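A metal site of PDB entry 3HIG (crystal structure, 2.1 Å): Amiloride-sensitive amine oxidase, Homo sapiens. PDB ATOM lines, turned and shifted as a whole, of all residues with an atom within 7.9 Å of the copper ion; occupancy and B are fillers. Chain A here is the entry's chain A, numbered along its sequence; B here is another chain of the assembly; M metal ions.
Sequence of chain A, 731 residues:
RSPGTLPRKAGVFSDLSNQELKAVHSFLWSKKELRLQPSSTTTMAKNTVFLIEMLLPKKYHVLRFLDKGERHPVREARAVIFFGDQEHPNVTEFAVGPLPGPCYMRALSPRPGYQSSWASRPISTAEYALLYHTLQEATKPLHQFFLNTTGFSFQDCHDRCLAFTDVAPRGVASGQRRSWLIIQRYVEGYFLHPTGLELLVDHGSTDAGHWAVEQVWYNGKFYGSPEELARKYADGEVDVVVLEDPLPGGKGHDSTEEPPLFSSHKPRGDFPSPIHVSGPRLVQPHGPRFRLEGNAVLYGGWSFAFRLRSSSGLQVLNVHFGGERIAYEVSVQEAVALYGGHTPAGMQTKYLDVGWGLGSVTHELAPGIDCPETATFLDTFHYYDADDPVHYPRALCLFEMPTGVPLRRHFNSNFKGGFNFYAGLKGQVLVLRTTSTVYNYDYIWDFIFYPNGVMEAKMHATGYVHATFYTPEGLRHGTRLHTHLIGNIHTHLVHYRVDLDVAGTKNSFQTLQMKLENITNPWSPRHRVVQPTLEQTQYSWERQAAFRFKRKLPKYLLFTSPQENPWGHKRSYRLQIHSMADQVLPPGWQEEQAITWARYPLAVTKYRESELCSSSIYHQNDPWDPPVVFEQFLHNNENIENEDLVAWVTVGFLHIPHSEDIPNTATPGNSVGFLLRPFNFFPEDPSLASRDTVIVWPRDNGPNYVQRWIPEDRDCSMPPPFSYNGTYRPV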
ATOM      1  N   ALA A 337      21.579  16.039  13.414  1.00  0.00           N
ATOM      2  CA  ALA A 337      22.766  16.787  13.662  1.00  0.00           C
ATOM      3  C   ALA A 337      22.855  17.006  15.199  1.00  0.00           C
ATOM      4  O   ALA A 337      21.970  17.636  15.817  1.00  0.00           O
ATOM      5  CB  ALA A 337      22.697  18.106  12.860  1.00  0.00           C
ATOM      6  N   TYR A 339      24.934  18.252  18.507  1.00  0.00           N
ATOM      7  CA  TYR A 339      25.894  19.321  18.743  1.00  0.00           C
ATOM      8  C   TYR A 339      26.472  19.265  20.145  1.00  0.00           C
ATOM      9  O   TYR A 339      25.895  18.651  21.054  1.00  0.00           O
ATOM     10  CB  TYR A 339      25.233  20.712  18.522  1.00  0.00           C
ATOM     11  CG  TYR A 339      25.039  21.035  17.045  1.00  0.00           C
ATOM     12  CD1 TYR A 339      26.004  21.744  16.332  1.00  0.00           C
ATOM     13  CD2 TYR A 339      23.931  20.576  16.361  1.00  0.00           C
ATOM     14  CE1 TYR A 339      25.845  22.004  14.989  1.00  0.00           C
ATOM     15  CE2 TYR A 339      23.768  20.824  15.012  1.00  0.00           C
ATOM     16  CZ  TYR A 339      24.708  21.528  14.323  1.00  0.00           C
ATOM     17  OH  TYR A 339      24.533  21.754  12.974  1.00  0.00           O
ATOM     18  N   ASN A 440      19.021  26.109   7.833  1.00  0.00           N
ATOM     19  CA  ASN A 440      20.352  26.605   7.460  1.00  0.00           C
ATOM     20  C   ASN A 440      21.058  25.695   6.469  1.00  0.00           C
ATOM     21  O   ASN A 440      21.731  26.193   5.562  1.00  0.00           O
ATOM     22  CB  ASN A 440      21.259  26.820   8.703  1.00  0.00           C
ATOM     23  CG  ASN A 440      21.350  25.601   9.603  1.00  0.00           C
ATOM     24  OD1 ASN A 440      20.345  25.132  10.132  1.00  0.00           O
ATOM     25  ND2 ASN A 440      22.562  25.079   9.774  1.00  0.00           N
ATOM     26  N   TPQ A 441      20.945  24.384   6.677  1.00  0.00           N
ATOM     27  CA  TPQ A 441      21.592  23.365   5.840  1.00  0.00           C
ATOM     28  CB  TPQ A 441      21.831  22.051   6.634  1.00  0.00           C
ATOM     29  C   TPQ A 441      20.742  22.991   4.628  1.00  0.00           C
ATOM     30  O   TPQ A 441      19.515  22.944   4.719  1.00  0.00           O
ATOM     31  C1  TPQ A 441      23.186  22.049   7.316  1.00  0.00           C
ATOM     32  C2  TPQ A 441      23.258  21.809   8.774  1.00  0.00           C
ATOM     33  O2  TPQ A 441      22.215  21.623   9.454  1.00  0.00           O
ATOM     34  C3  TPQ A 441      24.585  21.802   9.435  1.00  0.00           C
ATOM     35  C4  TPQ A 441      25.767  22.003   8.700  1.00  0.00           C
ATOM     36  O4  TPQ A 441      26.868  22.001   9.255  1.00  0.00           O
ATOM     37  C5  TPQ A 441      25.699  22.236   7.237  1.00  0.00           C
ATOM     38  O5  TPQ A 441      26.750  22.419   6.589  1.00  0.00           O
ATOM     39  C6  TPQ A 441      24.360  22.241   6.588  1.00  0.00           C
ATOM     40  N   TYR A 443      20.492  19.685   2.318  1.00  0.00           N
ATOM     41  CA  TYR A 443      20.905  18.333   2.041  1.00  0.00           C
ATOM     42  C   TYR A 443      20.454  17.953   0.646  1.00  0.00           C
ATOM     43  O   TYR A 443      19.293  18.160   0.281  1.00  0.00           O
ATOM     44  CB  TYR A 443      20.308  17.358   3.053  1.00  0.00           C
ATOM     45  CG  TYR A 443      20.798  17.508   4.465  1.00  0.00           C
ATOM     46  CD1 TYR A 443      22.119  17.885   4.752  1.00  0.00           C
ATOM     47  CD2 TYR A 443      19.945  17.231   5.541  1.00  0.00           C
ATOM     48  CE1 TYR A 443      22.558  18.007   6.075  1.00  0.00           C
ATOM     49  CE2 TYR A 443      20.377  17.343   6.871  1.00  0.00           C
ATOM     50  CZ  TYR A 443      21.685  17.730   7.131  1.00  0.00           C
ATOM     51  OH  TYR A 443      22.112  17.835   8.445  1.00  0.00           O
ATOM     52  N   ALA A 461      25.972  17.362   1.959  1.00  0.00           N
ATOM     53  CA  ALA A 461      25.634  18.496   2.841  1.00  0.00           C
ATOM     54  C   ALA A 461      26.205  19.804   2.295  1.00  0.00           C
ATOM     55  O   ALA A 461      27.391  19.874   1.958  1.00  0.00           O
ATOM     56  CB  ALA A 461      26.165  18.252   4.236  1.00  0.00           C
ATOM     57  N   THR A 462      25.370  20.834   2.148  1.00  0.00           N
ATOM     58  CA  THR A 462      25.848  22.187   1.881  1.00  0.00           C
ATOM     59  C   THR A 462      24.949  23.217   2.618  1.00  0.00           C
ATOM     60  O   THR A 462      24.208  22.851   3.504  1.00  0.00           O
ATOM     61  CB  THR A 462      26.032  22.421   0.351  1.00  0.00           C
ATOM     62  OG1 THR A 462      26.600  23.731   0.094  1.00  0.00           O
ATOM     63  CG2 THR A 462      24.714  22.243  -0.391  1.00  0.00           C
ATOM     64  N   TYR A 464      24.464  26.606   5.223  1.00  0.00           N
ATOM     65  CA  TYR A 464      25.115  27.319   6.339  1.00  0.00           C
ATOM     66  C   TYR A 464      25.212  26.456   7.573  1.00  0.00           C
ATOM     67  O   TYR A 464      24.268  25.730   7.871  1.00  0.00           O
ATOM     68  CB  TYR A 464      24.255  28.532   6.724  1.00  0.00           C
ATOM     69  CG  TYR A 464      24.326  29.699   5.773  1.00  0.00           C
ATOM     70  CD1 TYR A 464      23.417  29.815   4.726  1.00  0.00           C
ATOM     71  CD2 TYR A 464      25.294  30.709   5.941  1.00  0.00           C
ATOM     72  CE1 TYR A 464      23.469  30.893   3.832  1.00  0.00           C
ATOM     73  CE2 TYR A 464      25.354  31.796   5.040  1.00  0.00           C
ATOM     74  CZ  TYR A 464      24.422  31.884   4.015  1.00  0.00           C
ATOM     75  OH  TYR A 464      24.443  32.929   3.141  1.00  0.00           O
ATOM     76  N   VAL A 465      26.320  26.576   8.323  1.00  0.00           N
ATOM     77  CA  VAL A 465      26.469  25.901   9.609  1.00  0.00           C
ATOM     78  C   VAL A 465      25.590  26.508  10.754  1.00  0.00           C
ATOM     79  O   VAL A 465      25.173  27.674  10.686  1.00  0.00           O
ATOM     80  CB  VAL A 465      27.958  25.817  10.091  1.00  0.00           C
ATOM     81  CG1 VAL A 465      28.841  25.178   9.020  1.00  0.00           C
ATOM     82  CG2 VAL A 465      28.521  27.199  10.473  1.00  0.00           C
ATOM     83  N   HIS A 466      25.295  25.682  11.750  1.00  0.00           N
ATOM     84  CA  HIS A 466      24.687  26.089  13.013  1.00  0.00           C
ATOM     85  C   HIS A 466      25.822  26.682  13.872  1.00  0.00           C
ATOM     86  O   HIS A 466      26.793  25.983  14.207  1.00  0.00           O
ATOM     87  CB  HIS A 466      24.040  24.853  13.645  1.00  0.00           C
ATOM     88  CG  HIS A 466      23.274  25.109  14.902  1.00  0.00           C
ATOM     89  ND1 HIS A 466      22.158  25.919  14.947  1.00  0.00           N
ATOM     90  CD2 HIS A 466      23.418  24.607  16.147  1.00  0.00           C
ATOM     91  CE1 HIS A 466      21.667  25.928  16.168  1.00  0.00           C
ATOM     92  NE2 HIS A 466      22.416  25.132  16.917  1.00  0.00           N
ATOM     93  N   ASN A 488      30.077  25.293  16.118  1.00  0.00           N
ATOM     94  CA  ASN A 488      29.995  24.178  17.041  1.00  0.00           C
ATOM     95  C   ASN A 488      30.275  22.825  16.379  1.00  0.00           C
ATOM     96  O   ASN A 488      29.773  22.544  15.264  1.00  0.00           O
ATOM     97  CB  ASN A 488      28.598  24.114  17.663  1.00  0.00           C
ATOM     98  CG  ASN A 488      28.249  25.383  18.449  1.00  0.00           C
ATOM     99  OD1 ASN A 488      28.153  26.469  17.879  1.00  0.00           O
ATOM    100  ND2 ASN A 488      28.007  25.244  19.751  1.00  0.00           N
ATOM    101  N   ILE A 489      31.061  22.021  17.072  1.00  0.00           N
ATOM    102  CA  ILE A 489      31.295  20.635  16.731  1.00  0.00           C
ATOM    103  C   ILE A 489      29.971  19.880  16.717  1.00  0.00           C
ATOM    104  O   ILE A 489      29.069  20.162  17.523  1.00  0.00           O
ATOM    105  CB  ILE A 489      32.242  19.992  17.734  1.00  0.00           C
ATOM    106  CG1 ILE A 489      32.693  18.607  17.250  1.00  0.00           C
ATOM    107  CG2 ILE A 489      31.599  19.932  19.122  1.00  0.00           C
ATOM    108  CD1 ILE A 489      33.905  18.024  18.044  1.00  0.00           C
ATOM    109  N   HIS A 490      29.832  18.948  15.780  1.00  0.00           N
ATOM    110  CA  HIS A 490      28.646  18.133  15.680  1.00  0.00           C
ATOM    111  C   HIS A 490      28.856  16.914  14.802  1.00  0.00           C
ATOM    112  O   HIS A 490      29.854  16.780  14.112  1.00  0.00           O
ATOM    113  CB  HIS A 490      27.474  18.971  15.138  1.00  0.00           C
ATOM    114  CG  HIS A 490      27.721  19.527  13.779  1.00  0.00           C
ATOM    115  ND1 HIS A 490      28.614  20.544  13.546  1.00  0.00           N
ATOM    116  CD2 HIS A 490      27.210  19.185  12.562  1.00  0.00           C
ATOM    117  CE1 HIS A 490      28.648  20.814  12.252  1.00  0.00           C
ATOM    118  NE2 HIS A 490      27.809  20.000  11.634  1.00  0.00           N
ATOM    119  N   THR A 491      27.894  16.000  14.848  1.00  0.00           N
ATOM    120  CA  THR A 491      27.899  14.849  13.955  1.00  0.00           C
ATOM    121  C   THR A 491      26.607  14.804  13.179  1.00  0.00           C
ATOM    122  O   THR A 491      25.540  14.951  13.759  1.00  0.00           O
ATOM    123  CB  THR A 491      28.117  13.544  14.778  1.00  0.00           C
ATOM    124  OG1 THR A 491      29.342  13.683  15.511  1.00  0.00           O
ATOM    125  CG2 THR A 491      28.219  12.333  13.908  1.00  0.00           C
ATOM    126  N   HIS A 492      26.725  14.601  11.865  1.00  0.00           N
ATOM    127  CA  HIS A 492      25.599  14.333  11.013  1.00  0.00           C
ATOM    128  C   HIS A 492      25.388  12.812  10.967  1.00  0.00           C
ATOM    129  O   HIS A 492      26.319  12.075  10.688  1.00  0.00           O
ATOM    130  CB  HIS A 492      25.873  14.789   9.606  1.00  0.00           C
ATOM    131  CG  HIS A 492      26.029  16.264   9.438  1.00  0.00           C
ATOM    132  ND1 HIS A 492      24.982  17.077   9.060  1.00  0.00           N
ATOM    133  CD2 HIS A 492      27.125  17.062   9.517  1.00  0.00           C
ATOM    134  CE1 HIS A 492      25.411  18.320   8.958  1.00  0.00           C
ATOM    135  NE2 HIS A 492      26.710  18.341   9.211  1.00  0.00           N
ATOM    136  N   PHE A 653      28.993  11.478   9.529  1.00  0.00           N
ATOM    137  CA  PHE A 653      30.313  12.082   9.713  1.00  0.00           C
ATOM    138  C   PHE A 653      30.345  13.148  10.797  1.00  0.00           C
ATOM    139  O   PHE A 653      29.374  13.924  10.976  1.00  0.00           O
ATOM    140  CB  PHE A 653      30.866  12.629   8.401  1.00  0.00           C
ATOM    141  CG  PHE A 653      30.067  13.760   7.776  1.00  0.00           C
ATOM    142  CD1 PHE A 653      30.454  15.086   7.943  1.00  0.00           C
ATOM    143  CD2 PHE A 653      28.996  13.495   6.930  1.00  0.00           C
ATOM    144  CE1 PHE A 653      29.759  16.124   7.334  1.00  0.00           C
ATOM    145  CE2 PHE A 653      28.298  14.517   6.323  1.00  0.00           C
ATOM    146  CZ  PHE A 653      28.678  15.848   6.518  1.00  0.00           C
ATOM    147  N   LEU A 654      31.459  13.156  11.517  1.00  0.00           N
ATOM    148  CA  LEU A 654      31.827  14.228  12.421  1.00  0.00           C
ATOM    149  C   LEU A 654      32.210  15.442  11.582  1.00  0.00           C
ATOM    150  O   LEU A 654      33.031  15.349  10.650  1.00  0.00           O
ATOM    151  CB  LEU A 654      33.023  13.830  13.331  1.00  0.00           C
ATOM    152  CG  LEU A 654      33.593  14.913  14.295  1.00  0.00           C
ATOM    153  CD1 LEU A 654      32.621  15.231  15.418  1.00  0.00           C
ATOM    154  CD2 LEU A 654      34.926  14.478  14.913  1.00  0.00           C
ATOM    155  N   HIS A 655      31.609  16.574  11.911  1.00  0.00           N
ATOM    156  CA  HIS A 655      31.938  17.846  11.284  1.00  0.00           C
ATOM    157  C   HIS A 655      32.484  18.803  12.377  1.00  0.00           C
ATOM    158  O   HIS A 655      31.739  19.265  13.250  1.00  0.00           O
ATOM    159  CB  HIS A 655      30.682  18.397  10.582  1.00  0.00           C
ATOM    160  CG  HIS A 655      30.888  19.693   9.858  1.00  0.00           C
ATOM    161  ND1 HIS A 655      29.837  20.366   9.254  1.00  0.00           N
ATOM    162  CD2 HIS A 655      31.990  20.440   9.644  1.00  0.00           C
ATOM    163  CE1 HIS A 655      30.298  21.492   8.713  1.00  0.00           C
ATOM    164  NE2 HIS A 655      31.608  21.550   8.918  1.00  0.00           N
ATOM    165  N   ILE A 656      33.783  19.076  12.299  1.00  0.00           N
ATOM    166  CA  ILE A 656      34.417  20.134  13.091  1.00  0.00           C
ATOM    167  C   ILE A 656      34.544  21.299  12.155  1.00  0.00           C
ATOM    168  O   ILE A 656      35.301  21.230  11.187  1.00  0.00           O
ATOM    169  CB  ILE A 656      35.809  19.731  13.592  1.00  0.00           C
ATOM    170  CG1 ILE A 656      35.699  18.534  14.531  1.00  0.00           C
ATOM    171  CG2 ILE A 656      36.512  20.959  14.251  1.00  0.00           C
ATOM    172  CD1 ILE A 656      37.055  17.816  14.816  1.00  0.00           C
ATOM    173  N   PRO A 657      33.774  22.369  12.391  1.00  0.00           N
ATOM    174  CA  PRO A 657      33.826  23.470  11.418  1.00  0.00           C
ATOM    175  C   PRO A 657      35.199  24.110  11.304  1.00  0.00           C
ATOM    176  O   PRO A 657      36.024  24.046  12.207  1.00  0.00           O
ATOM    177  CB  PRO A 657      32.780  24.449  11.962  1.00  0.00           C
ATOM    178  CG  PRO A 657      31.802  23.541  12.636  1.00  0.00           C
ATOM    179  CD  PRO A 657      32.635  22.524  13.308  1.00  0.00           C
ATOM    180  N   ASP A 661      34.346  26.728   5.754  1.00  0.00           N
ATOM    181  CA  ASP A 661      32.872  26.621   5.798  1.00  0.00           C
ATOM    182  C   ASP A 661      32.151  28.001   5.704  1.00  0.00           C
ATOM    183  O   ASP A 661      30.941  28.041   5.760  1.00  0.00           O
ATOM    184  CB  ASP A 661      32.374  25.918   7.074  1.00  0.00           C
ATOM    185  CG  ASP A 661      32.641  24.403   7.095  1.00  0.00           C
ATOM    186  OD1 ASP A 661      32.406  23.718   6.078  1.00  0.00           O
ATOM    187  OD2 ASP A 661      33.094  23.877   8.136  1.00  0.00           O
ATOM    188  N   THR A 665      29.201  25.420   3.947  1.00  0.00           N
ATOM    189  CA  THR A 665      29.857  24.133   3.790  1.00  0.00           C
ATOM    190  C   THR A 665      29.727  23.758   2.309  1.00  0.00           C
ATOM    191  O   THR A 665      28.691  24.042   1.695  1.00  0.00           O
ATOM    192  CB  THR A 665      29.187  23.050   4.624  1.00  0.00           C
ATOM    193  OG1 THR A 665      29.257  23.396   6.005  1.00  0.00           O
ATOM    194  CG2 THR A 665      29.871  21.689   4.399  1.00  0.00           C
ATOM    195  N   ASN A 670      32.147  15.858   1.330  1.00  0.00           N
ATOM    196  CA  ASN A 670      31.128  15.946   2.366  1.00  0.00           C
ATOM    197  C   ASN A 670      29.899  15.130   1.972  1.00  0.00           C
ATOM    198  O   ASN A 670      28.756  15.589   2.137  1.00  0.00           O
ATOM    199  CB  ASN A 670      30.716  17.406   2.644  1.00  0.00           C
ATOM    200  CG  ASN A 670      31.562  18.062   3.727  1.00  0.00           C
ATOM    201  OD1 ASN A 670      32.024  17.395   4.619  1.00  0.00           O
ATOM    202  ND2 ASN A 670      31.799  19.391   3.616  1.00  0.00           N
ATOM    203  N   TYR B 556      39.924  13.116  12.066  1.00  0.00           N
ATOM    204  CA  TYR B 556      40.642  14.280  11.512  1.00  0.00           C
ATOM    205  C   TYR B 556      42.151  14.057  11.557  1.00  0.00           C
ATOM    206  O   TYR B 556      42.759  14.025  12.633  1.00  0.00           O
ATOM    207  CB  TYR B 556      40.247  15.563  12.254  1.00  0.00           C
ATOM    208  CG  TYR B 556      38.938  16.106  11.762  1.00  0.00           C
ATOM    209  CD1 TYR B 556      37.754  15.463  12.069  1.00  0.00           C
ATOM    210  CD2 TYR B 556      38.885  17.245  10.963  1.00  0.00           C
ATOM    211  CE1 TYR B 556      36.521  15.940  11.610  1.00  0.00           C
ATOM    212  CE2 TYR B 556      37.662  17.734  10.475  1.00  0.00           C
ATOM    213  CZ  TYR B 556      36.495  17.074  10.804  1.00  0.00           C
ATOM    214  OH  TYR B 556      35.277  17.523  10.340  1.00  0.00           O
HETATM  215 CU    CU M   1      27.922  19.953   9.567  1.00  0.00          CU
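NE2 of His 655 is in hydrogen-bond range of OD2 of Asp 661. The backbone carbonyl oxygen of Phe 653 is in hydrogen-bond range of the backbone NH of His 492 (2.9 Å). ND1 of His 492 is in hydrogen-bond range of OH of Tyr 443 (3.0 Å). A ring nitrogen (ND1) of His 490 sits at hydrogen-bond distance from the backbone carbonyl oxygen of Asn 488. O5 of TPQ 441 sits at hydrogen-bond distance from OG1 of Thr 665 (2.8 Å). O2 of TPQ 441 sits at hydrogen-bond distance from the side-chain amide nitrogen (ND2) of Asn 440 (3.5 Å).
Within 4 Å of the copper ion: TPQ 441, His 490, His 492 and His 655. The nearest printed residue that does not touch the copper ion is Phe 653 (4.8 Å).
The copper ion is bound by a ring nitrogen (ND1) of His 655 (2.0 Å), a ring nitrogen (NE2) of His 492 (2.0 Å), a ring nitrogen (NE2) of His 490 (2.1 Å) and O4 of TPQ 441 (2.3 Å). The copper ion has four donor atoms within binding distance.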
